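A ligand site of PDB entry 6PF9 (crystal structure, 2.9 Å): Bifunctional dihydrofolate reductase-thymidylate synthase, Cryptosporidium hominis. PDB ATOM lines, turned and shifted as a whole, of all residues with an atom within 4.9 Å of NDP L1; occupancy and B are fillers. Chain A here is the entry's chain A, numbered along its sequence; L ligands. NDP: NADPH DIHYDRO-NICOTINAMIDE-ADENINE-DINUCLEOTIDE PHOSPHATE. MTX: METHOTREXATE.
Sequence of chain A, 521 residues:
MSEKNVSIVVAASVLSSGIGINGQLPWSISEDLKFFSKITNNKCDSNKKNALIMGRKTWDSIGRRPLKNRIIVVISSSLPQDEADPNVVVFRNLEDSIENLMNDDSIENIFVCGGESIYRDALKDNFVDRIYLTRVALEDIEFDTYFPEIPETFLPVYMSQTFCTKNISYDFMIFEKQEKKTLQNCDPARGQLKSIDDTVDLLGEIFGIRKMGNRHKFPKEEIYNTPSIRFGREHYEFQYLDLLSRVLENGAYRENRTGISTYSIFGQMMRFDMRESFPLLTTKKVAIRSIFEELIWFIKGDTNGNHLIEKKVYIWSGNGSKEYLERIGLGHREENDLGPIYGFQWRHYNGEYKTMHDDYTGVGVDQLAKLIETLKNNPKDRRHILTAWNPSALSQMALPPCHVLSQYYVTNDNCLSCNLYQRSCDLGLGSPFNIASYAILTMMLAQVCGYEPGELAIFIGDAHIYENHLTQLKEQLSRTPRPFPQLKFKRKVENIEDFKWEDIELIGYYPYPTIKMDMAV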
ATOM      1  N   VAL A   9       3.169  -7.201  -8.116  1.00  0.00           N
ATOM      2  CA  VAL A   9       3.147  -7.969  -9.356  1.00  0.00           C
ATOM      3  C   VAL A   9       2.404  -9.262  -9.084  1.00  0.00           C
ATOM      4  O   VAL A   9       2.710  -9.963  -8.111  1.00  0.00           O
ATOM      5  CB  VAL A   9       4.573  -8.250  -9.878  1.00  0.00           C
ATOM      6  CG1 VAL A   9       4.520  -8.791 -11.299  1.00  0.00           C
ATOM      7  CG2 VAL A   9       5.428  -6.991  -9.794  1.00  0.00           C
ATOM      8  N   VAL A  10       1.421  -9.576  -9.924  1.00  0.00           N
ATOM      9  CA  VAL A  10       0.557 -10.725  -9.689  1.00  0.00           C
ATOM     10  C   VAL A  10      -0.060 -11.147 -11.010  1.00  0.00           C
ATOM     11  O   VAL A  10      -0.251 -10.328 -11.919  1.00  0.00           O
ATOM     12  CB  VAL A  10      -0.521 -10.403  -8.623  1.00  0.00           C
ATOM     13  CG1 VAL A  10      -1.443  -9.293  -9.101  1.00  0.00           C
ATOM     14  CG2 VAL A  10      -1.320 -11.651  -8.252  1.00  0.00           C
ATOM     15  N   ALA A  11      -0.363 -12.445 -11.125  1.00  0.00           N
ATOM     16  CA  ALA A  11      -1.114 -12.999 -12.250  1.00  0.00           C
ATOM     17  C   ALA A  11      -2.308 -13.750 -11.686  1.00  0.00           C
ATOM     18  O   ALA A  11      -2.146 -14.819 -11.078  1.00  0.00           O
ATOM     19  CB  ALA A  11      -0.239 -13.924 -13.099  1.00  0.00           C
ATOM     20  N   ILE A  19      -4.852 -17.468  -8.095  1.00  0.00           N
ATOM     21  CA  ILE A  19      -3.439 -17.283  -8.409  1.00  0.00           C
ATOM     22  C   ILE A  19      -2.626 -18.558  -8.164  1.00  0.00           C
ATOM     23  O   ILE A  19      -1.473 -18.650  -8.592  1.00  0.00           O
ATOM     24  CB  ILE A  19      -2.842 -16.110  -7.611  1.00  0.00           C
ATOM     25  CG1 ILE A  19      -2.846 -16.414  -6.106  1.00  0.00           C
ATOM     26  CG2 ILE A  19      -3.587 -14.824  -7.903  1.00  0.00           C
ATOM     27  CD1 ILE A  19      -2.153 -15.368  -5.278  1.00  0.00           C
ATOM     28  N   GLY A  20      -3.211 -19.536  -7.472  1.00  0.00           N
ATOM     29  CA  GLY A  20      -2.450 -20.731  -7.148  1.00  0.00           C
ATOM     30  C   GLY A  20      -3.336 -21.920  -6.842  1.00  0.00           C
ATOM     31  O   GLY A  20      -4.529 -21.781  -6.579  1.00  0.00           O
ATOM     32  N   ILE A  21      -2.717 -23.099  -6.883  1.00  0.00           N
ATOM     33  CA  ILE A  21      -3.387 -24.364  -6.568  1.00  0.00           C
ATOM     34  C   ILE A  21      -2.356 -25.417  -6.171  1.00  0.00           C
ATOM     35  O   ILE A  21      -1.424 -25.706  -6.925  1.00  0.00           O
ATOM     36  CB  ILE A  21      -4.249 -24.843  -7.740  1.00  0.00           C
ATOM     37  CG1 ILE A  21      -4.818 -26.236  -7.447  1.00  0.00           C
ATOM     38  CG2 ILE A  21      -3.465 -24.835  -9.046  1.00  0.00           C
ATOM     39  CD1 ILE A  21      -5.785 -26.272  -6.283  1.00  0.00           C
ATOM     40  N   GLY A  23       0.110 -25.432  -4.094  1.00  0.00           N
ATOM     41  CA  GLY A  23       1.482 -24.977  -4.011  1.00  0.00           C
ATOM     42  C   GLY A  23       2.136 -24.677  -5.333  1.00  0.00           C
ATOM     43  O   GLY A  23       3.364 -24.610  -5.402  1.00  0.00           O
ATOM     44  N   GLN A  24       1.361 -24.492  -6.403  1.00  0.00           N
ATOM     45  CA  GLN A  24       1.920 -24.159  -7.697  1.00  0.00           C
ATOM     46  C   GLN A  24       0.908 -23.329  -8.477  1.00  0.00           C
ATOM     47  O   GLN A  24      -0.241 -23.152  -8.056  1.00  0.00           O
ATOM     48  CB  GLN A  24       2.314 -25.417  -8.488  1.00  0.00           C
ATOM     49  CG  GLN A  24       1.154 -26.349  -8.790  1.00  0.00           C
ATOM     50  CD  GLN A  24       1.576 -27.592  -9.555  1.00  0.00           C
ATOM     51  OE1 GLN A  24       2.770 -27.813  -9.779  1.00  0.00           O
ATOM     52  NE2 GLN A  24       0.610 -28.390  -9.964  1.00  0.00           N
ATOM     53  N   LEU A  25       1.360 -22.807  -9.623  1.00  0.00           N
ATOM     54  CA  LEU A  25       0.494 -21.995 -10.468  1.00  0.00           C
ATOM     55  C   LEU A  25      -0.503 -22.871 -11.212  1.00  0.00           C
ATOM     56  O   LEU A  25      -0.194 -24.004 -11.596  1.00  0.00           O
ATOM     57  CB  LEU A  25       1.326 -21.200 -11.470  1.00  0.00           C
ATOM     58  CG  LEU A  25       2.440 -20.330 -10.907  1.00  0.00           C
ATOM     59  CD1 LEU A  25       3.274 -19.741 -12.036  1.00  0.00           C
ATOM     60  CD2 LEU A  25       1.875 -19.231 -10.024  1.00  0.00           C
ATOM     61  N   TRP A  27      -1.404 -22.512 -14.189  1.00  0.00           N
ATOM     62  CA  TRP A  27      -1.147 -22.375 -15.624  1.00  0.00           C
ATOM     63  C   TRP A  27       0.359 -22.277 -15.837  1.00  0.00           C
ATOM     64  O   TRP A  27       1.124 -22.010 -14.908  1.00  0.00           O
ATOM     65  CB  TRP A  27      -1.850 -21.148 -16.202  1.00  0.00           C
ATOM     66  CG  TRP A  27      -1.579 -19.887 -15.430  1.00  0.00           C
ATOM     67  CD1 TRP A  27      -0.405 -19.209 -15.351  1.00  0.00           C
ATOM     68  CD2 TRP A  27      -2.517 -19.170 -14.616  1.00  0.00           C
ATOM     69  NE1 TRP A  27      -0.538 -18.114 -14.535  1.00  0.00           N
ATOM     70  CE2 TRP A  27      -1.830 -18.062 -14.081  1.00  0.00           C
ATOM     71  CE3 TRP A  27      -3.859 -19.345 -14.299  1.00  0.00           C
ATOM     72  CZ2 TRP A  27      -2.444 -17.137 -13.235  1.00  0.00           C
ATOM     73  CZ3 TRP A  27      -4.468 -18.434 -13.462  1.00  0.00           C
ATOM     74  CH2 TRP A  27      -3.767 -17.341 -12.940  1.00  0.00           C
ATOM     75  N   GLY A  55       6.052 -14.423   0.351  1.00  0.00           N
ATOM     76  CA  GLY A  55       5.823 -15.291   1.484  1.00  0.00           C
ATOM     77  C   GLY A  55       6.687 -16.545   1.423  1.00  0.00           C
ATOM     78  O   GLY A  55       7.367 -16.832   0.438  1.00  0.00           O
ATOM     79  N   ARG A  56       6.644 -17.316   2.523  1.00  0.00           N
ATOM     80  CA  ARG A  56       7.476 -18.505   2.601  1.00  0.00           C
ATOM     81  C   ARG A  56       7.017 -19.572   1.618  1.00  0.00           C
ATOM     82  O   ARG A  56       7.844 -20.225   0.967  1.00  0.00           O
ATOM     83  CB  ARG A  56       7.478 -19.073   4.018  1.00  0.00           C
ATOM     84  CG  ARG A  56       8.605 -20.066   4.265  1.00  0.00           C
ATOM     85  CD  ARG A  56       8.211 -21.162   5.243  1.00  0.00           C
ATOM     86  NE  ARG A  56       7.412 -22.213   4.619  1.00  0.00           N
ATOM     87  CZ  ARG A  56       6.149 -22.508   4.936  1.00  0.00           C
ATOM     88  NH1 ARG A  56       5.533 -21.805   5.880  1.00  0.00           N
ATOM     89  NH2 ARG A  56       5.519 -23.482   4.313  1.00  0.00           N
ATOM     90  N   LYS A  57       5.700 -19.780   1.507  1.00  0.00           N
ATOM     91  CA  LYS A  57       5.193 -20.812   0.599  1.00  0.00           C
ATOM     92  C   LYS A  57       5.505 -20.479  -0.852  1.00  0.00           C
ATOM     93  O   LYS A  57       5.755 -21.380  -1.656  1.00  0.00           O
ATOM     94  CB  LYS A  57       3.691 -20.996   0.814  1.00  0.00           C
ATOM     95  CG  LYS A  57       3.338 -21.464   2.216  1.00  0.00           C
ATOM     96  CD  LYS A  57       1.884 -21.890   2.332  1.00  0.00           C
ATOM     97  CE  LYS A  57       1.589 -22.440   3.728  1.00  0.00           C
ATOM     98  NZ  LYS A  57       0.199 -22.945   3.870  1.00  0.00           N
ATOM     99  N   THR A  58       5.507 -19.184  -1.201  1.00  0.00           N
ATOM    100  CA  THR A  58       5.962 -18.782  -2.530  1.00  0.00           C
ATOM    101  C   THR A  58       7.463 -19.026  -2.672  1.00  0.00           C
ATOM    102  O   THR A  58       7.937 -19.439  -3.738  1.00  0.00           O
ATOM    103  CB  THR A  58       5.630 -17.310  -2.767  1.00  0.00           C
ATOM    104  OG1 THR A  58       4.205 -17.130  -2.726  1.00  0.00           O
ATOM    105  CG2 THR A  58       6.149 -16.842  -4.116  1.00  0.00           C
ATOM    106  N   SER A  61       7.858 -22.359  -3.680  1.00  0.00           N
ATOM    107  CA  SER A  61       7.406 -22.612  -5.043  1.00  0.00           C
ATOM    108  C   SER A  61       8.524 -22.400  -6.067  1.00  0.00           C
ATOM    109  O   SER A  61       8.539 -23.071  -7.111  1.00  0.00           O
ATOM    110  CB  SER A  61       6.214 -21.724  -5.390  1.00  0.00           C
ATOM    111  OG  SER A  61       5.113 -22.021  -4.549  1.00  0.00           O
ATOM    112  N   ILE A  75       9.223 -13.478   3.835  1.00  0.00           N
ATOM    113  CA  ILE A  75       8.461 -13.226   5.051  1.00  0.00           C
ATOM    114  C   ILE A  75       8.114 -14.579   5.659  1.00  0.00           C
ATOM    115  O   ILE A  75       7.336 -15.345   5.084  1.00  0.00           O
ATOM    116  CB  ILE A  75       7.195 -12.407   4.770  1.00  0.00           C
ATOM    117  CG1 ILE A  75       7.548 -11.064   4.112  1.00  0.00           C
ATOM    118  CG2 ILE A  75       6.394 -12.179   6.045  1.00  0.00           C
ATOM    119  CD1 ILE A  75       8.513 -10.235   4.911  1.00  0.00           C
ATOM    120  N   SER A  76       8.686 -14.875   6.816  1.00  0.00           N
ATOM    121  CA  SER A  76       8.426 -16.147   7.485  1.00  0.00           C
ATOM    122  C   SER A  76       8.787 -16.025   8.954  1.00  0.00           C
ATOM    123  O   SER A  76       9.777 -15.377   9.309  1.00  0.00           O
ATOM    124  CB  SER A  76       9.222 -17.291   6.841  1.00  0.00           C
ATOM    125  OG  SER A  76       8.956 -18.518   7.491  1.00  0.00           O
ATOM    126  N   SER A  77       7.972 -16.648   9.811  1.00  0.00           N
ATOM    127  CA  SER A  77       8.220 -16.653  11.246  1.00  0.00           C
ATOM    128  C   SER A  77       9.095 -17.816  11.689  1.00  0.00           C
ATOM    129  O   SER A  77       9.561 -17.826  12.832  1.00  0.00           O
ATOM    130  CB  SER A  77       6.898 -16.683  12.011  1.00  0.00           C
ATOM    131  OG  SER A  77       6.114 -17.801  11.614  1.00  0.00           O
ATOM    132  N   SER A  78       9.319 -18.808  10.831  1.00  0.00           N
ATOM    133  CA  SER A  78      10.073 -20.002  11.185  1.00  0.00           C
ATOM    134  C   SER A  78      11.432 -20.094  10.508  1.00  0.00           C
ATOM    135  O   SER A  78      12.347 -20.691  11.091  1.00  0.00           O
ATOM    136  CB  SER A  78       9.271 -21.263  10.843  1.00  0.00           C
ATOM    137  OG  SER A  78       9.074 -21.390   9.443  1.00  0.00           O
ATOM    138  N   ARG A  92      10.653 -11.242  10.010  1.00  0.00           N
ATOM    139  CA  ARG A  92       9.629 -11.915  10.788  1.00  0.00           C
ATOM    140  C   ARG A  92       8.222 -11.457  10.416  1.00  0.00           C
ATOM    141  O   ARG A  92       7.277 -12.264  10.505  1.00  0.00           O
ATOM    142  CB  ARG A  92       9.863 -11.680  12.278  1.00  0.00           C
ATOM    143  CG  ARG A  92      11.154 -12.298  12.799  1.00  0.00           C
ATOM    144  CD  ARG A  92      11.212 -13.775  12.455  1.00  0.00           C
ATOM    145  NE  ARG A  92      12.559 -14.322  12.629  1.00  0.00           N
ATOM    146  CZ  ARG A  92      12.919 -15.560  12.292  1.00  0.00           C
ATOM    147  NH1 ARG A  92      12.026 -16.381  11.750  1.00  0.00           N
ATOM    148  NH2 ARG A  92      14.155 -15.970  12.490  1.00  0.00           N
ATOM    149  N   ASN A  93       8.040 -10.210  10.010  1.00  0.00           N
ATOM    150  CA  ASN A  93       6.742  -9.692   9.619  1.00  0.00           C
ATOM    151  C   ASN A  93       6.919  -8.759   8.421  1.00  0.00           C
ATOM    152  O   ASN A  93       8.028  -8.334   8.094  1.00  0.00           O
ATOM    153  CB  ASN A  93       6.041  -8.973  10.782  1.00  0.00           C
ATOM    154  CG  ASN A  93       6.850  -7.815  11.322  1.00  0.00           C
ATOM    155  OD1 ASN A  93       6.949  -6.755  10.690  1.00  0.00           O
ATOM    156  ND2 ASN A  93       7.436  -8.000  12.505  1.00  0.00           N
ATOM    157  N   CYS A 113       5.584  -9.558  -4.677  1.00  0.00           N
ATOM    158  CA  CYS A 113       5.082 -10.678  -5.456  1.00  0.00           C
ATOM    159  C   CYS A 113       4.907 -11.917  -4.577  1.00  0.00           C
ATOM    160  O   CYS A 113       5.444 -12.981  -4.891  1.00  0.00           O
ATOM    161  CB  CYS A 113       6.022 -10.967  -6.634  1.00  0.00           C
ATOM    162  SG  CYS A 113       7.762 -11.055  -6.160  1.00  0.00           S
ATOM    163  N   GLY A 114       4.151 -11.786  -3.495  1.00  0.00           N
ATOM    164  CA  GLY A 114       3.933 -12.864  -2.555  1.00  0.00           C
ATOM    165  C   GLY A 114       2.648 -13.621  -2.845  1.00  0.00           C
ATOM    166  O   GLY A 114       2.185 -13.688  -3.990  1.00  0.00           O
ATOM    167  N   GLY A 115       2.068 -14.200  -1.796  1.00  0.00           N
ATOM    168  CA  GLY A 115       0.829 -14.919  -1.904  1.00  0.00           C
ATOM    169  C   GLY A 115      -0.343 -14.153  -1.317  1.00  0.00           C
ATOM    170  O   GLY A 115      -0.254 -12.957  -1.011  1.00  0.00           O
ATOM    171  N   GLU A 116      -1.461 -14.866  -1.184  1.00  0.00           N
ATOM    172  CA  GLU A 116      -2.673 -14.257  -0.622  1.00  0.00           C
ATOM    173  C   GLU A 116      -2.411 -13.674   0.755  1.00  0.00           C
ATOM    174  O   GLU A 116      -2.926 -12.599   1.088  1.00  0.00           O
ATOM    175  CB  GLU A 116      -3.796 -15.297  -0.565  1.00  0.00           C
ATOM    176  CG  GLU A 116      -5.127 -14.760  -0.061  1.00  0.00           C
ATOM    177  CD  GLU A 116      -6.257 -15.765  -0.232  1.00  0.00           C
ATOM    178  OE1 GLU A 116      -6.039 -16.827  -0.837  1.00  0.00           O
ATOM    179  OE2 GLU A 116      -7.380 -15.479   0.259  1.00  0.00           O
ATOM    180  N   SER A 117      -1.613 -14.361   1.579  1.00  0.00           N
ATOM    181  CA  SER A 117      -1.293 -13.855   2.908  1.00  0.00           C
ATOM    182  C   SER A 117      -0.505 -12.555   2.822  1.00  0.00           C
ATOM    183  O   SER A 117      -0.726 -11.635   3.613  1.00  0.00           O
ATOM    184  CB  SER A 117      -0.515 -14.909   3.698  1.00  0.00           C
ATOM    185  OG  SER A 117       0.725 -15.196   3.087  1.00  0.00           O
ATOM    186  N   ILE A 118       0.438 -12.465   1.874  1.00  0.00           N
ATOM    187  CA  ILE A 118       1.257 -11.272   1.758  1.00  0.00           C
ATOM    188  C   ILE A 118       0.512 -10.168   1.000  1.00  0.00           C
ATOM    189  O   ILE A 118       0.616  -8.992   1.358  1.00  0.00           O
ATOM    190  CB  ILE A 118       2.605 -11.615   1.085  1.00  0.00           C
ATOM    191  CG1 ILE A 118       3.324 -12.707   1.878  1.00  0.00           C
ATOM    192  CG2 ILE A 118       3.489 -10.370   0.994  1.00  0.00           C
ATOM    193  CD1 ILE A 118       3.630 -12.336   3.308  1.00  0.00           C
ATOM    194  N   TYR A 119      -0.233 -10.535  -0.043  1.00  0.00           N
ATOM    195  CA  TYR A 119      -0.989  -9.542  -0.803  1.00  0.00           C
ATOM    196  C   TYR A 119      -2.020  -8.844   0.075  1.00  0.00           C
ATOM    197  O   TYR A 119      -2.197  -7.624  -0.004  1.00  0.00           O
ATOM    198  CB  TYR A 119      -1.685 -10.205  -1.996  1.00  0.00           C
ATOM    199  CG  TYR A 119      -0.783 -10.544  -3.150  1.00  0.00           C
ATOM    200  CD1 TYR A 119       0.269  -9.704  -3.509  1.00  0.00           C
ATOM    201  CD2 TYR A 119      -0.994 -11.699  -3.896  1.00  0.00           C
ATOM    202  CE1 TYR A 119       1.095 -10.028  -4.575  1.00  0.00           C
ATOM    203  CE2 TYR A 119      -0.177 -12.021  -4.958  1.00  0.00           C
ATOM    204  CZ  TYR A 119       0.862 -11.176  -5.299  1.00  0.00           C
ATOM    205  OH  TYR A 119       1.679 -11.499  -6.360  1.00  0.00           O
ATOM    206  N   ASP A 121      -2.383  -8.304   3.490  1.00  0.00           N
ATOM    207  CA  ASP A 121      -1.908  -7.341   4.477  1.00  0.00           C
ATOM    208  C   ASP A 121      -0.841  -6.397   3.919  1.00  0.00           C
ATOM    209  O   ASP A 121      -0.210  -5.677   4.692  1.00  0.00           O
ATOM    210  CB  ASP A 121      -1.381  -8.078   5.715  1.00  0.00           C
ATOM    211  CG  ASP A 121      -0.370  -9.151   5.387  1.00  0.00           C
ATOM    212  OD1 ASP A 121       0.224  -9.112   4.294  1.00  0.00           O
ATOM    213  OD2 ASP A 121      -0.171 -10.046   6.241  1.00  0.00           O
ATOM    214  N   THR A 145      -5.948 -20.426  -3.707  1.00  0.00           N
ATOM    215  CA  THR A 145      -5.286 -19.193  -3.282  1.00  0.00           C
ATOM    216  C   THR A 145      -5.662 -18.101  -4.265  1.00  0.00           C
ATOM    217  O   THR A 145      -5.467 -18.258  -5.467  1.00  0.00           O
ATOM    218  CB  THR A 145      -3.758 -19.370  -3.220  1.00  0.00           C
ATOM    219  OG1 THR A 145      -3.431 -20.380  -2.260  1.00  0.00           O
ATOM    220  CG2 THR A 145      -3.088 -18.065  -2.834  1.00  0.00           C
HETATM  221  PA  NDP L   1       2.378 -17.249   0.850  1.00  0.00           P
HETATM  222  O1A NDP L   1       1.499 -16.012   0.929  1.00  0.00           O
HETATM  223  O2A NDP L   1       3.228 -17.172  -0.390  1.00  0.00           O
HETATM  224  O5B NDP L   1       3.298 -17.276   2.072  1.00  0.00           O
HETATM  225  C5B NDP L   1       2.852 -17.799   3.291  1.00  0.00           C
HETATM  226  C4B NDP L   1       3.810 -17.788   4.409  1.00  0.00           C
HETATM  227  O4B NDP L   1       4.250 -16.465   4.645  1.00  0.00           O
HETATM  228  C3B NDP L   1       3.218 -18.211   5.679  1.00  0.00           C
HETATM  229  O3B NDP L   1       3.202 -19.587   5.810  1.00  0.00           O
HETATM  230  C2B NDP L   1       4.095 -17.596   6.648  1.00  0.00           C
HETATM  231  O2B NDP L   1       5.294 -18.316   6.768  1.00  0.00           O
HETATM  232  C1B NDP L   1       4.409 -16.308   6.053  1.00  0.00           C
HETATM  233  N9A NDP L   1       3.522 -15.309   6.557  1.00  0.00           N
HETATM  234  C8A NDP L   1       2.348 -14.923   6.018  1.00  0.00           C
HETATM  235  N7A NDP L   1       1.804 -13.951   6.774  1.00  0.00           N
HETATM  236  C5A NDP L   1       2.648 -13.707   7.831  1.00  0.00           C
HETATM  237  C6A NDP L   1       2.620 -12.815   8.938  1.00  0.00           C
HETATM  238  N6A NDP L   1       1.464 -11.892   9.109  1.00  0.00           N
HETATM  239  N1A NDP L   1       3.640 -12.821   9.837  1.00  0.00           N
HETATM  240  C2A NDP L   1       4.685 -13.673   9.660  1.00  0.00           C
HETATM  241  N3A NDP L   1       4.751 -14.525   8.637  1.00  0.00           N
HETATM  242  C4A NDP L   1       3.738 -14.569   7.695  1.00  0.00           C
HETATM  243  O3  NDP L   1       1.468 -18.557   0.798  1.00  0.00           O
HETATM  244  PN  NDP L   1       0.270 -18.715  -0.230  1.00  0.00           P
HETATM  245  O1N NDP L   1      -0.362 -20.112  -0.113  1.00  0.00           O
HETATM  246  O2N NDP L   1      -0.789 -17.669   0.075  1.00  0.00           O
HETATM  247  O5D NDP L   1       0.808 -18.521  -1.746  1.00  0.00           O
HETATM  248  C5D NDP L   1       1.298 -19.633  -2.452  1.00  0.00           C
HETATM  249  C4D NDP L   1       0.619 -20.004  -3.685  1.00  0.00           C
HETATM  250  O4D NDP L   1       0.359 -18.847  -4.467  1.00  0.00           O
HETATM  251  C3D NDP L   1       1.464 -20.881  -4.515  1.00  0.00           C
HETATM  252  O3D NDP L   1       0.657 -21.750  -5.249  1.00  0.00           O
HETATM  253  C2D NDP L   1       2.115 -19.988  -5.406  1.00  0.00           C
HETATM  254  O2D NDP L   1       2.500 -20.669  -6.565  1.00  0.00           O
HETATM  255  C1D NDP L   1       1.045 -18.996  -5.674  1.00  0.00           C
HETATM  256  N1N NDP L   1       1.595 -17.757  -6.120  1.00  0.00           N
HETATM  257  C2N NDP L   1       1.071 -17.180  -7.218  1.00  0.00           C
HETATM  258  C3N NDP L   1       1.571 -15.966  -7.710  1.00  0.00           C
HETATM  259  C7N NDP L   1       0.949 -15.363  -8.951  1.00  0.00           C
HETATM  260  O7N NDP L   1       1.303 -14.226  -9.319  1.00  0.00           O
HETATM  261  N7N NDP L   1      -0.056 -16.066  -9.699  1.00  0.00           N
HETATM  262  C4N NDP L   1       2.640 -15.331  -7.042  1.00  0.00           C
HETATM  263  C5N NDP L   1       3.158 -15.958  -5.904  1.00  0.00           C
HETATM  264  C6N NDP L   1       2.636 -17.159  -5.455  1.00  0.00           C
HETATM  265  P2B NDP L   1       5.601 -19.165   8.041  1.00  0.00           P
HETATM  266  O1X NDP L   1       4.393 -20.091   8.319  1.00  0.00           O
HETATM  267  O2X NDP L   1       6.812 -19.959   7.823  1.00  0.00           O
HETATM  268  O3X NDP L   1       5.830 -18.265   9.218  1.00  0.00           O
HETATM  269  N1  MTX L   2       3.285 -13.990 -12.716  1.00  0.00           N
HETATM  270  C2  MTX L   2       3.031 -12.671 -12.557  1.00  0.00           C
HETATM  271  NA2 MTX L   2       2.439 -11.943 -13.638  1.00  0.00           N
HETATM  272  N3  MTX L   2       3.318 -12.019 -11.418  1.00  0.00           N
HETATM  273  C4  MTX L   2       3.885 -12.668 -10.375  1.00  0.00           C
HETATM  274  NA4 MTX L   2       4.193 -11.983  -9.163  1.00  0.00           N
HETATM  275  C4A MTX L   2       4.168 -14.054 -10.492  1.00  0.00           C
HETATM  276  N5  MTX L   2       4.733 -14.742  -9.465  1.00  0.00           N
HETATM  277  C6  MTX L   2       4.974 -16.065  -9.627  1.00  0.00           C
HETATM  278  C7  MTX L   2       4.672 -16.737 -10.810  1.00  0.00           C
HETATM  279  N8  MTX L   2       4.115 -16.031 -11.825  1.00  0.00           N
HETATM  280  C8A MTX L   2       3.852 -14.688 -11.685  1.00  0.00           C
HETATM  281  C9  MTX L   2       5.610 -16.826  -8.481  1.00  0.00           C
HETATM  282  N10 MTX L   2       6.442 -17.936  -8.897  1.00  0.00           N
HETATM  283  CM  MTX L   2       6.106 -19.287  -8.499  1.00  0.00           C
HETATM  284  C11 MTX L   2       9.847 -17.300 -11.356  1.00  0.00           C
HETATM  285  C12 MTX L   2       9.116 -18.477 -11.439  1.00  0.00           C
HETATM  286  C13 MTX L   2       8.006 -18.669 -10.632  1.00  0.00           C
HETATM  287  C14 MTX L   2       7.612 -17.692  -9.728  1.00  0.00           C
HETATM  288  C15 MTX L   2       8.348 -16.510  -9.637  1.00  0.00           C
HETATM  289  C16 MTX L   2       9.466 -16.310 -10.453  1.00  0.00           C
HETATM  290  C   MTX L   2      11.050 -17.107 -12.244  1.00  0.00           C
HETATM  291  O   MTX L   2      11.699 -18.088 -12.578  1.00  0.00           O
HETATM  292  N   MTX L   2      11.447 -15.806 -12.730  1.00  0.00           N
HETATM  293  CA  MTX L   2      12.604 -15.672 -13.587  1.00  0.00           C
HETATM  294  CT  MTX L   2      13.239 -14.371 -13.306  1.00  0.00           C
HETATM  295  O1  MTX L   2      12.772 -13.647 -12.385  1.00  0.00           O
HETATM  296  O2  MTX L   2      14.245 -13.985 -13.982  1.00  0.00           O
HETATM  297  CB  MTX L   2      12.144 -15.668 -15.010  1.00  0.00           C
HETATM  298  CG  MTX L   2      12.298 -16.901 -15.847  1.00  0.00           C
HETATM  299  CD  MTX L   2      12.180 -16.702 -17.328  1.00  0.00           C
HETATM  300  OE1 MTX L   2      12.651 -15.665 -17.842  1.00  0.00           O
HETATM  301  OE2 MTX L   2      11.347 -17.385 -17.975  1.00  0.00           O
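OG of Ser 77 sits at hydrogen-bond distance from O3X of NDP L1 (2.5 Å). The side-chain hydroxyl of Thr 58 is in hydrogen-bond range of an oxygen (O2A) of NDP L1 (2.5 Å). N of Glu 116 sits at hydrogen-bond distance from O2N of NDP L1 (3.1 Å). N of Gln 24 sits at hydrogen-bond distance from O3D of NDP L1. The backbone carbonyl oxygen (O) of Ala 11 is in hydrogen-bond range of a nitrogen (N7N) of NDP L1, at 2.8 Å. N of Ser 77 lies within hydrogen-bond range of O3X of NDP L1, 2.7 Å away. N of Val 10 is in hydrogen-bond range of N3 of MTX L2 (3.4 Å). The backbone NH of Thr 58 sits at hydrogen-bond distance from an oxygen (O2A) of NDP L1, 3.1 Å away. The backbone carbonyl oxygen (O) of Val 9 is in hydrogen-bond range of a nitrogen (NA4) of MTX L2 (2.7 Å). O1A of NDP L1 is in hydrogen-bond range of OG of Ser 117. The guanidinium group of Arg 56 lies within salt-bridge range of an oxygen (O2X) of NDP L1. N of Ala 11 sits at hydrogen-bond distance from O7N of NDP L1 (3.0 Å). The backbone NH (N) of Gly 115 lies close to an oxygen (O1A) of NDP L1 (3.3 Å). N7N of NDP L1 lies within hydrogen-bond range of O of Ile 19, at 3.1 Å. N of Arg 56 is in hydrogen-bond range of O4B of NDP L1. OG of Ser 78 sits at hydrogen-bond distance from O2X of NDP L1. An oxygen (O2X) of NDP L1 is in hydrogen-bond range of the side-chain hydroxyl (OG) of Ser 76 (2.6 Å). An oxygen (O3D) of NDP L1 lies within hydrogen-bond range of the backbone carbonyl oxygen of Gln 24, at 3.3 Å.
The backbone NH (N) of Arg 56 lies within hydrogen-bond range of the backbone carbonyl oxygen (O) of Ile 75 (3.3 Å). OG of Ser 61 lies within hydrogen-bond range of O of Lys 57, 3.0 Å away. The side-chain hydroxyl of Ser 76 sits at hydrogen-bond distance from the backbone NH of Ser 78 (3.4 Å). O of Thr 145 lies within hydrogen-bond range of N of Gly 20 (3.3 Å). The backbone carbonyl oxygen (O) of Gly 114 sits close to the side-chain hydroxyl (OH) of Tyr 119 (3.3 Å). The guanidinium group of Arg 92 sits at hydrogen-bond distance from the backbone carbonyl oxygen of Ser 76 (3.5 Å). O of Gly 23 sits at hydrogen-bond distance from OG of Ser 61, at 3.2 Å. N of Ile 19 sits at hydrogen-bond distance from O of Thr 145 (2.8 Å).
An oxygen (O4B) of NDP L1 lies close to the backbone carbonyl oxygen (O) of Ile 75 (3.3 Å). CA of Val 10 touches O7N of NDP L1, 3.6 Å away. Gly 20 touches NDP L1. Ile 21 touches NDP L1 (N to O3D, 3.98 Å). C of Gly 23 touches O3D of NDP L1, at 3.3 Å. Leu 25 touches NDP L1 (CD2 to C2N, 3.6 Å). Gly 55 touches NDP L1. Lys 57 touches NDP L1 (CB to O3, 3.3 Å). Ser 61 touches NDP L1 (OG to O2D, 3.6 Å). Arg 92 touches NDP L1 (O to C2A, 3.1 Å). O of Cys 113 touches C5N of NDP L1, 3.9 Å away. O of Gly 114 touches C5N of NDP L1, 3.1 Å away. Ile 118 touches NDP L1 (N to O1A, 3.8 Å). Asp 121 touches NDP L1 (OD2 to N6A, 3.8 Å). Thr 145 touches NDP L1. Hydrophobic or aromatic side chains within 4 Å of NDP L1: Val 10, Ile 19, Leu 25, Ile 75 and Ile 118. Within 4 Å of NDP L1: Val 10, Ala 11, Ile 19, Gly 20, Ile 21, Gly 23, Gln 24, Leu 25, Gly 55, Arg 56, Lys 57, Thr 58, Ser 61, Ile 75, Ser 76, Ser 77, Ser 78, Arg 92, Cys 113, Gly 114, Gly 115, Glu 116, Ser 117, Ile 118, Asp 121 and Thr 145.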
